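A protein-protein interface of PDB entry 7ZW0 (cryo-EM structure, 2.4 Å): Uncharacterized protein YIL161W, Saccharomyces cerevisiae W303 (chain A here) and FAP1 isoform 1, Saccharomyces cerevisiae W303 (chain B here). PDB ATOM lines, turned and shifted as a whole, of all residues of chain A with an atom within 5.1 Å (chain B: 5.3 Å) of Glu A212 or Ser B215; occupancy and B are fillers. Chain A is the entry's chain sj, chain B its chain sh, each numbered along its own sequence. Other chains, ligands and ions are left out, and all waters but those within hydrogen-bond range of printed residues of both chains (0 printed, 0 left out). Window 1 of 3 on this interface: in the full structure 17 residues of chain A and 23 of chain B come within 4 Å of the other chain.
Of the printed residues of chain B, Asn A207 touches Pro B213 and Ser B215.
Printed residues of chain B within 4 Å of Tyr A208: Ser B215 (3.9 Å).
Printed residues of chain B within 4 Å of Ser A211: Ser B215.
Glu A212 touches one residue of chain B.
Of the printed residues of chain A, Pro B213 touches Asn A207 (3.9 Å).
Of chain A, only Asn A207, Tyr A208, Ser A211 and Glu A212 come within 4 Å of Ser B215.
ND2 of Asn A207 touches O of Pro B213, at 3.9 Å.
Ser B215 touches Asn A207.
Ser B215 touches Tyr A208 (O to CD1, 3.9 Å).
CB of Ser A211 touches OG of Ser B215, 3.3 Å away.
CB of Ser B215 touches OE1 of Glu A212, at 3.1 Å.
Of the 7 printed residues of chain B, 2 touch a printed residue of chain A.
Hydrophobic or aromatic side chains of chain A that line the printed part of chain B: Tyr A208.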
ATOM      1  N   ASN A 207       1.300 -17.515   2.311  1.00  0.00           N
ATOM      2  CA  ASN A 207       1.734 -16.803   3.509  1.00  0.00           C
ATOM      3  C   ASN A 207       1.384 -17.585   4.769  1.00  0.00           C
ATOM      4  O   ASN A 207       2.168 -17.627   5.722  1.00  0.00           O
ATOM      5  CB  ASN A 207       1.104 -15.411   3.546  1.00  0.00           C
ATOM      6  CG  ASN A 207       1.570 -14.596   4.732  1.00  0.00           C
ATOM      7  OD1 ASN A 207       2.739 -14.218   4.816  1.00  0.00           O
ATOM      8  ND2 ASN A 207       0.660 -14.320   5.658  1.00  0.00           N
ATOM      9  N   TYR A 208       0.212 -18.223   4.772  1.00  0.00           N
ATOM     10  CA  TYR A 208      -0.241 -19.057   5.880  1.00  0.00           C
ATOM     11  C   TYR A 208       0.730 -20.219   6.100  1.00  0.00           C
ATOM     12  O   TYR A 208       1.163 -20.501   7.232  1.00  0.00           O
ATOM     13  CB  TYR A 208      -1.647 -19.540   5.501  1.00  0.00           C
ATOM     14  CG  TYR A 208      -2.462 -20.385   6.448  1.00  0.00           C
ATOM     15  CD1 TYR A 208      -3.094 -19.811   7.543  1.00  0.00           C
ATOM     16  CD2 TYR A 208      -2.640 -21.742   6.224  1.00  0.00           C
ATOM     17  CE1 TYR A 208      -3.878 -20.569   8.394  1.00  0.00           C
ATOM     18  CE2 TYR A 208      -3.406 -22.513   7.078  1.00  0.00           C
ATOM     19  CZ  TYR A 208      -4.019 -21.921   8.164  1.00  0.00           C
ATOM     20  OH  TYR A 208      -4.783 -22.682   9.017  1.00  0.00           O
ATOM     21  N   LEU A 209       1.128 -20.855   4.994  1.00  0.00           N
ATOM     22  CA  LEU A 209       2.085 -21.956   4.991  1.00  0.00           C
ATOM     23  C   LEU A 209       3.449 -21.529   5.519  1.00  0.00           C
ATOM     24  O   LEU A 209       4.025 -22.187   6.392  1.00  0.00           O
ATOM     25  CB  LEU A 209       2.217 -22.495   3.564  1.00  0.00           C
ATOM     26  CG  LEU A 209       3.120 -23.697   3.289  1.00  0.00           C
ATOM     27  CD1 LEU A 209       2.630 -24.926   4.021  1.00  0.00           C
ATOM     28  CD2 LEU A 209       3.199 -23.960   1.792  1.00  0.00           C
ATOM     29  N   VAL A 210       3.990 -20.429   4.989  1.00  0.00           N
ATOM     30  CA  VAL A 210       5.341 -20.031   5.377  1.00  0.00           C
ATOM     31  C   VAL A 210       5.331 -19.442   6.786  1.00  0.00           C
ATOM     32  O   VAL A 210       6.364 -19.398   7.466  1.00  0.00           O
ATOM     33  CB  VAL A 210       5.931 -19.053   4.340  1.00  0.00           C
ATOM     34  CG1 VAL A 210       5.198 -17.727   4.362  1.00  0.00           C
ATOM     35  CG2 VAL A 210       7.442 -18.876   4.512  1.00  0.00           C
ATOM     36  N   SER A 211       4.162 -19.012   7.263  1.00  0.00           N
ATOM     37  CA  SER A 211       4.057 -18.499   8.618  1.00  0.00           C
ATOM     38  C   SER A 211       4.045 -19.605   9.662  1.00  0.00           C
ATOM     39  O   SER A 211       4.773 -19.499  10.656  1.00  0.00           O
ATOM     40  CB  SER A 211       2.801 -17.642   8.757  1.00  0.00           C
ATOM     41  OG  SER A 211       2.767 -16.620   7.776  1.00  0.00           O
ATOM     42  N   GLU A 212       3.246 -20.659   9.480  1.00  0.00           N
ATOM     43  CA  GLU A 212       3.274 -21.752  10.450  1.00  0.00           C
ATOM     44  C   GLU A 212       3.612 -23.115   9.845  1.00  0.00           C
ATOM     45  O   GLU A 212       2.965 -24.116  10.172  1.00  0.00           O
ATOM     46  CB  GLU A 212       1.968 -21.791  11.255  1.00  0.00           C
ATOM     47  CG  GLU A 212       0.684 -22.056  10.506  1.00  0.00           C
ATOM     48  CD  GLU A 212       0.027 -20.781  10.086  1.00  0.00           C
ATOM     49  OE1 GLU A 212       0.698 -19.732  10.112  1.00  0.00           O
ATOM     50  OE2 GLU A 212      -1.169 -20.818   9.771  1.00  0.00           O
ATOM     51  N   LEU A 213       4.662 -23.188   9.025  1.00  0.00           N
ATOM     52  CA  LEU A 213       5.175 -24.484   8.586  1.00  0.00           C
ATOM     53  C   LEU A 213       5.746 -25.290   9.752  1.00  0.00           C
ATOM     54  O   LEU A 213       5.877 -26.516   9.663  1.00  0.00           O
ATOM     55  CB  LEU A 213       6.246 -24.298   7.508  1.00  0.00           C
ATOM     56  CG  LEU A 213       7.645 -23.771   7.866  1.00  0.00           C
ATOM     57  CD1 LEU A 213       8.583 -24.045   6.709  1.00  0.00           C
ATOM     58  CD2 LEU A 213       7.687 -22.289   8.218  1.00  0.00           C
ATOM     59  N   GLU A 214       6.103 -24.614  10.849  1.00  0.00           N
ATOM     60  CA  GLU A 214       6.646 -25.303  12.015  1.00  0.00           C
ATOM     61  C   GLU A 214       5.599 -26.157  12.722  1.00  0.00           C
ATOM     62  O   GLU A 214       5.938 -27.206  13.282  1.00  0.00           O
ATOM     63  CB  GLU A 214       7.241 -24.286  12.990  1.00  0.00           C
ATOM     64  CG  GLU A 214       8.631 -23.800  12.620  1.00  0.00           C
ATOM     65  CD  GLU A 214       9.644 -24.926  12.568  1.00  0.00           C
ATOM     66  OE1 GLU A 214       9.895 -25.546  13.622  1.00  0.00           O
ATOM     67  OE2 GLU A 214      10.190 -25.191  11.475  1.00  0.00           O
ATOM     68  N   ILE A 215       4.338 -25.733  12.719  1.00  0.00           N
ATOM     69  CA  ILE A 215       3.309 -26.473  13.441  1.00  0.00           C
ATOM     70  C   ILE A 215       2.591 -27.458  12.516  1.00  0.00           C
ATOM     71  O   ILE A 215       1.924 -28.385  12.989  1.00  0.00           O
ATOM     72  CB  ILE A 215       2.320 -25.489  14.101  1.00  0.00           C
ATOM     73  CG1 ILE A 215       1.478 -26.169  15.183  1.00  0.00           C
ATOM     74  CG2 ILE A 215       1.384 -24.897  13.064  1.00  0.00           C
ATOM     75  CD1 ILE A 215       2.283 -26.617  16.384  1.00  0.00           C
ATOM     76  N   LEU A 216       2.748 -27.301  11.198  1.00  0.00           N
ATOM     77  CA  LEU A 216       2.056 -28.167  10.247  1.00  0.00           C
ATOM     78  C   LEU A 216       2.650 -29.569  10.215  1.00  0.00           C
ATOM     79  O   LEU A 216       2.005 -30.502   9.723  1.00  0.00           O
ATOM     80  CB  LEU A 216       2.094 -27.538   8.856  1.00  0.00           C
ATOM     81  CG  LEU A 216       1.094 -26.405   8.634  1.00  0.00           C
ATOM     82  CD1 LEU A 216       1.496 -25.553   7.453  1.00  0.00           C
ATOM     83  CD2 LEU A 216      -0.280 -26.995   8.401  1.00  0.00           C
ATOM     84  N   PRO B 213      -4.826 -11.241   4.558  1.00  0.00           N
ATOM     85  CA  PRO B 213      -4.974 -11.721   5.930  1.00  0.00           C
ATOM     86  C   PRO B 213      -3.705 -12.344   6.444  1.00  0.00           C
ATOM     87  O   PRO B 213      -3.092 -13.174   5.775  1.00  0.00           O
ATOM     88  CB  PRO B 213      -6.065 -12.792   5.821  1.00  0.00           C
ATOM     89  CG  PRO B 213      -6.307 -12.998   4.358  1.00  0.00           C
ATOM     90  CD  PRO B 213      -5.893 -11.734   3.677  1.00  0.00           C
ATOM     91  N   LEU B 214      -3.317 -11.954   7.647  1.00  0.00           N
ATOM     92  CA  LEU B 214      -2.135 -12.524   8.260  1.00  0.00           C
ATOM     93  C   LEU B 214      -2.480 -13.922   8.712  1.00  0.00           C
ATOM     94  O   LEU B 214      -3.652 -14.251   8.845  1.00  0.00           O
ATOM     95  CB  LEU B 214      -1.632 -11.651   9.402  1.00  0.00           C
ATOM     96  CG  LEU B 214      -0.877 -10.423   8.890  1.00  0.00           C
ATOM     97  CD1 LEU B 214      -0.644  -9.354   9.945  1.00  0.00           C
ATOM     98  CD2 LEU B 214       0.423 -10.809   8.208  1.00  0.00           C
ATOM     99  N   SER B 215      -1.482 -14.742   8.982  1.00  0.00           N
ATOM    100  CA  SER B 215      -1.732 -16.147   9.299  1.00  0.00           C
ATOM    101  C   SER B 215      -2.625 -16.374  10.502  1.00  0.00           C
ATOM    102  O   SER B 215      -3.414 -17.317  10.516  1.00  0.00           O
ATOM    103  CB  SER B 215      -0.405 -16.854   9.498  1.00  0.00           C
ATOM    104  OG  SER B 215       0.428 -16.094  10.360  1.00  0.00           O
ATOM    105  N   CYS B 216      -2.518 -15.518  11.505  1.00  0.00           N
ATOM    106  CA  CYS B 216      -3.349 -15.646  12.684  1.00  0.00           C
ATOM    107  C   CYS B 216      -4.785 -15.572  12.243  1.00  0.00           C
ATOM    108  O   CYS B 216      -5.630 -16.193  12.886  1.00  0.00           O
ATOM    109  CB  CYS B 216      -3.057 -14.508  13.640  1.00  0.00           C
ATOM    110  SG  CYS B 216      -3.528 -12.883  13.016  1.00  0.00           S
ATOM    111  N   SER B 217      -5.074 -14.774  11.215  1.00  0.00           N
ATOM    112  CA  SER B 217      -6.425 -14.626  10.648  1.00  0.00           C
ATOM    113  C   SER B 217      -7.234 -13.602  11.402  1.00  0.00           C
ATOM    114  O   SER B 217      -8.358 -13.293  11.022  1.00  0.00           O
ATOM    115  CB  SER B 217      -7.181 -15.952  10.467  1.00  0.00           C
ATOM    116  OG  SER B 217      -8.287 -15.783   9.598  1.00  0.00           O
ATOM    117  N   PRO B 232       5.267 -12.834   8.671  1.00  0.00           N
ATOM    118  CA  PRO B 232       4.580 -13.214   9.911  1.00  0.00           C
ATOM    119  C   PRO B 232       3.695 -12.123  10.481  1.00  0.00           C
ATOM    120  O   PRO B 232       4.017 -10.949  10.337  1.00  0.00           O
ATOM    121  CB  PRO B 232       5.734 -13.488  10.883  1.00  0.00           C
ATOM    122  CG  PRO B 232       6.907 -12.763  10.314  1.00  0.00           C
ATOM    123  CD  PRO B 232       6.732 -12.820   8.826  1.00  0.00           C
ATOM    124  N   CYS B 233       2.588 -12.506  11.109  1.00  0.00           N
ATOM    125  CA  CYS B 233       1.751 -11.517  11.752  1.00  0.00           C
ATOM    126  C   CYS B 233       2.562 -10.918  12.871  1.00  0.00           C
ATOM    127  O   CYS B 233       3.109 -11.638  13.700  1.00  0.00           O
ATOM    128  CB  CYS B 233       0.515 -12.182  12.344  1.00  0.00           C
ATOM    129  SG  CYS B 233      -0.548 -11.032  13.238  1.00  0.00           S
